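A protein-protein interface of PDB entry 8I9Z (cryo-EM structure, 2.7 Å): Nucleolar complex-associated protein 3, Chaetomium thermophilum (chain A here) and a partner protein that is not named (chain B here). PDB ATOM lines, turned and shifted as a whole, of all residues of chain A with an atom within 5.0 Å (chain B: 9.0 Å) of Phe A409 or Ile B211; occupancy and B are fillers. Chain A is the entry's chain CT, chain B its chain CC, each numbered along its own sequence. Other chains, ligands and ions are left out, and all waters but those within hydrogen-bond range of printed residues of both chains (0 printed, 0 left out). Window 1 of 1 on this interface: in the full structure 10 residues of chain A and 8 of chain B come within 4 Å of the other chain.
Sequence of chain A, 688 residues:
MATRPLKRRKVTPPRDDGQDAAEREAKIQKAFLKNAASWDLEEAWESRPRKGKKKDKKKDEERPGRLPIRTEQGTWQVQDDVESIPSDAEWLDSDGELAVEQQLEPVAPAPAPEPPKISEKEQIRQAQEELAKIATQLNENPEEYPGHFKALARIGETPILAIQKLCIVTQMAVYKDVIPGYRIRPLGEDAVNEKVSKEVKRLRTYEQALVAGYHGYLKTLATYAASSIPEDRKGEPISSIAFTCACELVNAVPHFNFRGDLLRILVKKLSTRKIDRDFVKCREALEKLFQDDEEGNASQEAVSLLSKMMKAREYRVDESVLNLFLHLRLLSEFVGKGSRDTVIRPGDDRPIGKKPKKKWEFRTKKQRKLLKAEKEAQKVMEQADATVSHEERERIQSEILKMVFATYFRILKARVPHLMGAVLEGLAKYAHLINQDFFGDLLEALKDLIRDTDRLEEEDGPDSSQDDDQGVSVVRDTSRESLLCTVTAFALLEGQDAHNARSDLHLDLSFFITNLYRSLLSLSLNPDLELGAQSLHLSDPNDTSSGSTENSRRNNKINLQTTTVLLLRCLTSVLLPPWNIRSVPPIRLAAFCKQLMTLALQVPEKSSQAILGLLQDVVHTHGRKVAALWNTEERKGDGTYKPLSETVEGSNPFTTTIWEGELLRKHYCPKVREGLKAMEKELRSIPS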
ATOM      1  N   LYS A 402      21.234  24.206  12.536  1.00  0.00           N
ATOM      2  CA  LYS A 402      22.027  23.987  11.331  1.00  0.00           C
ATOM      3  C   LYS A 402      23.284  23.187  11.640  1.00  0.00           C
ATOM      4  O   LYS A 402      23.629  22.253  10.911  1.00  0.00           O
ATOM      5  CB  LYS A 402      22.390  25.319  10.674  1.00  0.00           C
ATOM      6  CG  LYS A 402      21.263  25.946   9.885  1.00  0.00           C
ATOM      7  CD  LYS A 402      21.708  27.224   9.204  1.00  0.00           C
ATOM      8  CE  LYS A 402      20.554  27.887   8.476  1.00  0.00           C
ATOM      9  NZ  LYS A 402      20.962  29.167   7.835  1.00  0.00           N
ATOM     10  N   PHE A 405      22.248  19.473  12.831  1.00  0.00           N
ATOM     11  CA  PHE A 405      21.777  18.588  11.773  1.00  0.00           C
ATOM     12  C   PHE A 405      22.850  18.325  10.725  1.00  0.00           C
ATOM     13  O   PHE A 405      22.824  17.277  10.071  1.00  0.00           O
ATOM     14  CB  PHE A 405      20.522  19.163  11.124  1.00  0.00           C
ATOM     15  CG  PHE A 405      19.249  18.628  11.702  1.00  0.00           C
ATOM     16  CD1 PHE A 405      18.798  19.060  12.931  1.00  0.00           C
ATOM     17  CD2 PHE A 405      18.524  17.666  11.034  1.00  0.00           C
ATOM     18  CE1 PHE A 405      17.637  18.557  13.469  1.00  0.00           C
ATOM     19  CE2 PHE A 405      17.362  17.161  11.567  1.00  0.00           C
ATOM     20  CZ  PHE A 405      16.920  17.605  12.785  1.00  0.00           C
ATOM     21  N   ALA A 406      23.793  19.252  10.543  1.00  0.00           N
ATOM     22  CA  ALA A 406      24.892  19.004   9.616  1.00  0.00           C
ATOM     23  C   ALA A 406      25.818  17.915  10.135  1.00  0.00           C
ATOM     24  O   ALA A 406      26.336  17.107   9.357  1.00  0.00           O
ATOM     25  CB  ALA A 406      25.675  20.287   9.356  1.00  0.00           C
ATOM     26  N   THR A 407      26.054  17.889  11.448  1.00  0.00           N
ATOM     27  CA  THR A 407      26.841  16.815  12.039  1.00  0.00           C
ATOM     28  C   THR A 407      26.107  15.487  11.936  1.00  0.00           C
ATOM     29  O   THR A 407      26.727  14.443  11.705  1.00  0.00           O
ATOM     30  CB  THR A 407      27.162  17.150  13.496  1.00  0.00           C
ATOM     31  OG1 THR A 407      27.820  18.420  13.555  1.00  0.00           O
ATOM     32  CG2 THR A 407      28.071  16.105  14.112  1.00  0.00           C
ATOM     33  N   TYR A 408      24.782  15.513  12.093  1.00  0.00           N
ATOM     34  CA  TYR A 408      23.977  14.302  11.983  1.00  0.00           C
ATOM     35  C   TYR A 408      24.073  13.694  10.589  1.00  0.00           C
ATOM     36  O   TYR A 408      24.244  12.479  10.437  1.00  0.00           O
ATOM     37  CB  TYR A 408      22.521  14.617  12.320  1.00  0.00           C
ATOM     38  CG  TYR A 408      22.220  14.735  13.793  1.00  0.00           C
ATOM     39  CD1 TYR A 408      21.003  15.230  14.227  1.00  0.00           C
ATOM     40  CD2 TYR A 408      23.148  14.349  14.748  1.00  0.00           C
ATOM     41  CE1 TYR A 408      20.717  15.341  15.566  1.00  0.00           C
ATOM     42  CE2 TYR A 408      22.870  14.457  16.092  1.00  0.00           C
ATOM     43  CZ  TYR A 408      21.653  14.955  16.494  1.00  0.00           C
ATOM     44  OH  TYR A 408      21.367  15.065  17.832  1.00  0.00           O
ATOM     45  N   PHE A 409      23.970  14.529   9.556  1.00  0.00           N
ATOM     46  CA  PHE A 409      23.947  14.009   8.196  1.00  0.00           C
ATOM     47  C   PHE A 409      25.334  13.611   7.717  1.00  0.00           C
ATOM     48  O   PHE A 409      25.456  12.778   6.813  1.00  0.00           O
ATOM     49  CB  PHE A 409      23.333  15.030   7.247  1.00  0.00           C
ATOM     50  CG  PHE A 409      21.910  15.361   7.561  1.00  0.00           C
ATOM     51  CD1 PHE A 409      21.066  14.403   8.086  1.00  0.00           C
ATOM     52  CD2 PHE A 409      21.410  16.622   7.312  1.00  0.00           C
ATOM     53  CE1 PHE A 409      19.758  14.703   8.374  1.00  0.00           C
ATOM     54  CE2 PHE A 409      20.102  16.923   7.596  1.00  0.00           C
ATOM     55  CZ  PHE A 409      19.277  15.963   8.127  1.00  0.00           C
ATOM     56  N   ARG A 410      26.383  14.191   8.292  1.00  0.00           N
ATOM     57  CA  ARG A 410      27.731  13.793   7.906  1.00  0.00           C
ATOM     58  C   ARG A 410      28.101  12.451   8.523  1.00  0.00           C
ATOM     59  O   ARG A 410      28.915  11.707   7.964  1.00  0.00           O
ATOM     60  CB  ARG A 410      28.731  14.872   8.304  1.00  0.00           C
ATOM     61  CG  ARG A 410      28.951  15.911   7.229  1.00  0.00           C
ATOM     62  CD  ARG A 410      29.896  17.006   7.693  1.00  0.00           C
ATOM     63  NE  ARG A 410      29.785  18.226   6.902  1.00  0.00           N
ATOM     64  CZ  ARG A 410      30.174  18.362   5.641  1.00  0.00           C
ATOM     65  NH1 ARG A 410      30.784  17.383   4.990  1.00  0.00           N
ATOM     66  NH2 ARG A 410      29.964  19.517   5.019  1.00  0.00           N
ATOM     67  N   ILE A 411      27.524  12.131   9.679  1.00  0.00           N
ATOM     68  CA  ILE A 411      27.705  10.810  10.270  1.00  0.00           C
ATOM     69  C   ILE A 411      26.968   9.764   9.451  1.00  0.00           C
ATOM     70  O   ILE A 411      27.485   8.668   9.201  1.00  0.00           O
ATOM     71  CB  ILE A 411      27.236  10.820  11.736  1.00  0.00           C
ATOM     72  CG1 ILE A 411      28.182  11.666  12.575  1.00  0.00           C
ATOM     73  CG2 ILE A 411      27.170   9.416  12.298  1.00  0.00           C
ATOM     74  CD1 ILE A 411      27.699  11.937  13.966  1.00  0.00           C
ATOM     75  N   LEU A 412      25.756  10.094   9.008  1.00  0.00           N
ATOM     76  CA  LEU A 412      24.964   9.157   8.223  1.00  0.00           C
ATOM     77  C   LEU A 412      25.606   8.893   6.867  1.00  0.00           C
ATOM     78  O   LEU A 412      25.443   7.810   6.294  1.00  0.00           O
ATOM     79  CB  LEU A 412      23.547   9.696   8.061  1.00  0.00           C
ATOM     80  CG  LEU A 412      22.643   9.578   9.288  1.00  0.00           C
ATOM     81  CD1 LEU A 412      21.229  10.010   8.953  1.00  0.00           C
ATOM     82  CD2 LEU A 412      22.658   8.172   9.849  1.00  0.00           C
ATOM     83  N   LYS A 413      26.340   9.871   6.337  1.00  0.00           N
ATOM     84  CA  LYS A 413      27.057   9.659   5.086  1.00  0.00           C
ATOM     85  C   LYS A 413      28.313   8.824   5.296  1.00  0.00           C
ATOM     86  O   LYS A 413      28.645   7.972   4.465  1.00  0.00           O
ATOM     87  CB  LYS A 413      27.413  10.999   4.450  1.00  0.00           C
ATOM     88  CG  LYS A 413      26.583  11.348   3.230  1.00  0.00           C
ATOM     89  CD  LYS A 413      26.886  12.750   2.725  1.00  0.00           C
ATOM     90  CE  LYS A 413      28.315  12.906   2.226  1.00  0.00           C
ATOM     91  NZ  LYS A 413      28.876  11.677   1.595  1.00  0.00           N
ATOM     92  N   LEU A 427      17.787  12.673  15.617  1.00  0.00           N
ATOM     93  CA  LEU A 427      16.957  13.003  14.464  1.00  0.00           C
ATOM     94  C   LEU A 427      15.478  12.867  14.791  1.00  0.00           C
ATOM     95  O   LEU A 427      14.673  13.718  14.405  1.00  0.00           O
ATOM     96  CB  LEU A 427      17.328  12.103  13.289  1.00  0.00           C
ATOM     97  CG  LEU A 427      17.096  12.632  11.881  1.00  0.00           C
ATOM     98  CD1 LEU A 427      18.328  13.373  11.414  1.00  0.00           C
ATOM     99  CD2 LEU A 427      16.775  11.488  10.943  1.00  0.00           C
ATOM    100  N   LEU A 442      13.711  13.682   5.239  1.00  0.00           N
ATOM    101  CA  LEU A 442      14.228  12.771   6.254  1.00  0.00           C
ATOM    102  C   LEU A 442      13.600  11.395   6.114  1.00  0.00           C
ATOM    103  O   LEU A 442      14.262  10.371   6.313  1.00  0.00           O
ATOM    104  CB  LEU A 442      13.967  13.338   7.646  1.00  0.00           C
ATOM    105  CG  LEU A 442      14.718  14.610   8.023  1.00  0.00           C
ATOM    106  CD1 LEU A 442      13.981  15.345   9.125  1.00  0.00           C
ATOM    107  CD2 LEU A 442      16.122  14.268   8.459  1.00  0.00           C
ATOM    108  N   ASP B 202      23.029  11.642  -3.883  1.00  0.00           N
ATOM    109  CA  ASP B 202      22.489  11.017  -2.686  1.00  0.00           C
ATOM    110  C   ASP B 202      21.508  11.949  -1.987  1.00  0.00           C
ATOM    111  O   ASP B 202      21.616  13.175  -2.067  1.00  0.00           O
ATOM    112  CB  ASP B 202      23.620  10.635  -1.732  1.00  0.00           C
ATOM    113  CG  ASP B 202      23.221   9.542  -0.763  1.00  0.00           C
ATOM    114  OD1 ASP B 202      22.075   9.055  -0.849  1.00  0.00           O
ATOM    115  OD2 ASP B 202      24.057   9.170   0.088  1.00  0.00           O
ATOM    116  N   ALA B 203      20.532  11.349  -1.304  1.00  0.00           N
ATOM    117  CA  ALA B 203      19.557  12.135  -0.555  1.00  0.00           C
ATOM    118  C   ALA B 203      20.206  12.831   0.632  1.00  0.00           C
ATOM    119  O   ALA B 203      19.808  13.940   1.006  1.00  0.00           O
ATOM    120  CB  ALA B 203      18.408  11.243  -0.088  1.00  0.00           C
ATOM    121  N   LEU B 204      21.199  12.184   1.247  1.00  0.00           N
ATOM    122  CA  LEU B 204      21.954  12.827   2.315  1.00  0.00           C
ATOM    123  C   LEU B 204      22.785  13.983   1.778  1.00  0.00           C
ATOM    124  O   LEU B 204      22.989  14.985   2.471  1.00  0.00           O
ATOM    125  CB  LEU B 204      22.846  11.802   3.009  1.00  0.00           C
ATOM    126  CG  LEU B 204      22.168  10.839   3.978  1.00  0.00           C
ATOM    127  CD1 LEU B 204      23.125   9.744   4.372  1.00  0.00           C
ATOM    128  CD2 LEU B 204      21.679  11.578   5.205  1.00  0.00           C
ATOM    129  N   GLN B 205      23.287  13.857   0.546  1.00  0.00           N
ATOM    130  CA  GLN B 205      24.021  14.955  -0.072  1.00  0.00           C
ATOM    131  C   GLN B 205      23.110  16.137  -0.369  1.00  0.00           C
ATOM    132  O   GLN B 205      23.490  17.289  -0.139  1.00  0.00           O
ATOM    133  CB  GLN B 205      24.711  14.484  -1.349  1.00  0.00           C
ATOM    134  CG  GLN B 205      25.797  15.426  -1.838  1.00  0.00           C
ATOM    135  CD  GLN B 205      26.776  15.806  -0.751  1.00  0.00           C
ATOM    136  OE1 GLN B 205      27.518  14.965  -0.247  1.00  0.00           O
ATOM    137  NE2 GLN B 205      26.785  17.080  -0.385  1.00  0.00           N
ATOM    138  N   ASN B 206      21.906  15.873  -0.877  1.00  0.00           N
ATOM    139  CA  ASN B 206      20.975  16.956  -1.178  1.00  0.00           C
ATOM    140  C   ASN B 206      20.485  17.629   0.094  1.00  0.00           C
ATOM    141  O   ASN B 206      20.213  18.834   0.105  1.00  0.00           O
ATOM    142  CB  ASN B 206      19.793  16.427  -1.987  1.00  0.00           C
ATOM    143  CG  ASN B 206      20.222  15.735  -3.255  1.00  0.00           C
ATOM    144  OD1 ASN B 206      21.217  16.111  -3.873  1.00  0.00           O
ATOM    145  ND2 ASN B 206      19.475  14.713  -3.653  1.00  0.00           N
ATOM    146  N   LEU B 207      20.360  16.867   1.174  1.00  0.00           N
ATOM    147  CA  LEU B 207      19.882  17.435   2.424  1.00  0.00           C
ATOM    148  C   LEU B 207      20.969  18.239   3.125  1.00  0.00           C
ATOM    149  O   LEU B 207      20.661  19.086   3.969  1.00  0.00           O
ATOM    150  CB  LEU B 207      19.343  16.315   3.315  1.00  0.00           C
ATOM    151  CG  LEU B 207      18.329  16.676   4.393  1.00  0.00           C
ATOM    152  CD1 LEU B 207      17.259  17.582   3.824  1.00  0.00           C
ATOM    153  CD2 LEU B 207      17.697  15.409   4.922  1.00  0.00           C
ATOM    154  N   LEU B 208      22.237  17.998   2.785  1.00  0.00           N
ATOM    155  CA  LEU B 208      23.317  18.836   3.295  1.00  0.00           C
ATOM    156  C   LEU B 208      23.387  20.166   2.557  1.00  0.00           C
ATOM    157  O   LEU B 208      23.722  21.195   3.155  1.00  0.00           O
ATOM    158  CB  LEU B 208      24.651  18.102   3.193  1.00  0.00           C
ATOM    159  CG  LEU B 208      25.077  17.252   4.385  1.00  0.00           C
ATOM    160  CD1 LEU B 208      26.280  16.416   4.017  1.00  0.00           C
ATOM    161  CD2 LEU B 208      25.398  18.140   5.561  1.00  0.00           C
ATOM    162  N   ASP B 209      23.090  20.168   1.255  1.00  0.00           N
ATOM    163  CA  ASP B 209      23.082  21.423   0.509  1.00  0.00           C
ATOM    164  C   ASP B 209      21.899  22.293   0.906  1.00  0.00           C
ATOM    165  O   ASP B 209      21.938  23.518   0.747  1.00  0.00           O
ATOM    166  CB  ASP B 209      23.061  21.161  -0.996  1.00  0.00           C
ATOM    167  CG  ASP B 209      23.950  20.010  -1.400  1.00  0.00           C
ATOM    168  OD1 ASP B 209      24.994  19.807  -0.746  1.00  0.00           O
ATOM    169  OD2 ASP B 209      23.608  19.306  -2.373  1.00  0.00           O
ATOM    170  N   SER B 210      20.833  21.676   1.412  1.00  0.00           N
ATOM    171  CA  SER B 210      19.697  22.446   1.898  1.00  0.00           C
ATOM    172  C   SER B 210      20.049  23.200   3.173  1.00  0.00           C
ATOM    173  O   SER B 210      19.544  24.304   3.410  1.00  0.00           O
ATOM    174  CB  SER B 210      18.505  21.523   2.130  1.00  0.00           C
ATOM    175  OG  SER B 210      18.462  20.497   1.156  1.00  0.00           O
ATOM    176  N   ILE B 211      20.909  22.620   4.009  1.00  0.00           N
ATOM    177  CA  ILE B 211      21.271  23.259   5.270  1.00  0.00           C
ATOM    178  C   ILE B 211      22.474  24.172   5.078  1.00  0.00           C
ATOM    179  O   ILE B 211      22.392  25.389   5.279  1.00  0.00           O
ATOM    180  CB  ILE B 211      21.540  22.197   6.346  1.00  0.00           C
ATOM    181  CG1 ILE B 211      20.267  21.394   6.591  1.00  0.00           C
ATOM    182  CG2 ILE B 211      22.038  22.853   7.625  1.00  0.00           C
ATOM    183  CD1 ILE B 211      20.345  20.478   7.759  1.00  0.00           C
ATOM    184  N   GLU B 212      23.603  23.601   4.686  1.00  0.00           N
ATOM    185  CA  GLU B 212      24.811  24.357   4.383  1.00  0.00           C
ATOM    186  C   GLU B 212      24.874  24.497   2.866  1.00  0.00           C
ATOM    187  O   GLU B 212      25.340  23.602   2.161  1.00  0.00           O
ATOM    188  CB  GLU B 212      26.046  23.671   4.949  1.00  0.00           C
ATOM    189  CG  GLU B 212      25.956  23.391   6.438  1.00  0.00           C
ATOM    190  CD  GLU B 212      27.166  22.650   6.969  1.00  0.00           C
ATOM    191  OE1 GLU B 212      27.795  21.902   6.193  1.00  0.00           O
ATOM    192  OE2 GLU B 212      27.491  22.822   8.163  1.00  0.00           O
ATOM    193  N   VAL B 213      24.381  25.630   2.376  1.00  0.00           N
ATOM    194  CA  VAL B 213      24.282  25.927   0.950  1.00  0.00           C
ATOM    195  C   VAL B 213      25.691  26.050   0.383  1.00  0.00           C
ATOM    196  O   VAL B 213      26.570  26.613   1.051  1.00  0.00           O
ATOM    197  CB  VAL B 213      23.463  27.207   0.721  1.00  0.00           C
ATOM    198  CG1 VAL B 213      22.896  27.251  -0.676  1.00  0.00           C
ATOM    199  CG2 VAL B 213      22.346  27.310   1.743  1.00  0.00           C
ATOM    200  N   PRO B 214      25.961  25.523  -0.812  1.00  0.00           N
ATOM    201  CA  PRO B 214      27.296  25.672  -1.400  1.00  0.00           C
ATOM    202  C   PRO B 214      27.624  27.122  -1.727  1.00  0.00           C
ATOM    203  O   PRO B 214      26.750  27.983  -1.830  1.00  0.00           O
ATOM    204  CB  PRO B 214      27.221  24.820  -2.671  1.00  0.00           C
ATOM    205  CG  PRO B 214      26.144  23.849  -2.404  1.00  0.00           C
ATOM    206  CD  PRO B 214      25.140  24.567  -1.568  1.00  0.00           C
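Printed residues of chain B within 4 Å of Lys A402: Ile B211.
Ala A406 touches just one residue of chain B: Glu B212.
Tyr A408 touches none of the printed residues of chain B.
Phe A409 touches two residues of chain B.
Printed residues of chain B within 4 Å of Leu A412: Leu B204.
Asp B202 touches none of the printed residues of chain A.
Printed residues of chain A within 4 Å of Leu B207: Phe A409.
Of the printed residues of chain A, Leu B208 touches Lys A413 (3.9 Å).
Of chain A, only Lys A402 (3.7 Å), Phe A405 (3.6 Å) and Phe A409 (3.6 Å) come within 4 Å of Ile B211.
The nearest residue of chain B that does not touch Phe A409 is Leu B208 (4.02 Å).
OD1 of Asp B209 is in hydrogen-bond range of NE2 of Gln B205 (3.3 Å).
Hydrophobic or aromatic side chains of chain B within 4 Å of the printed part of chain A: Leu B204, Leu B207, Leu B208 and Ile B211.
Of the 12 printed residues of chain A, 7 touch a printed residue of chain B.
Hydrophobic or aromatic side chains of chain A that line the printed part of chain B: Phe A405, Ala A406, Phe A409 and Leu A412.
Among the printed residues, 10 pairs touch across the chains.
Among the printed residues, Asp or Glu carboxylates within 4 Å of a Lys or Arg side-chain nitrogen of the other chain: Arg A410 with Glu B212.
Lys A402 touches Ile B211.
Phe A405 touches Ile B211.
CB of Ala A406 touches OE2 of Glu B212 (3.3 Å).
Phe A409 touches Leu B207 (CZ to CD2, 3.6 Å).
Phe A409 touches Ile B211 (CE2 to CD1, 3.6 Å).
Leu B204 touches Leu A412.
Lys A413 touches Leu B204 (N to CD1, 3.8 Å).
Gln B205 touches Lys A413.
Leu B208 touches Lys A413.
The side-chain carboxylate (OE1) of Glu B212 is in salt-bridge range of the guanidinium group (NH2) of Arg A410 (3.4 Å).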
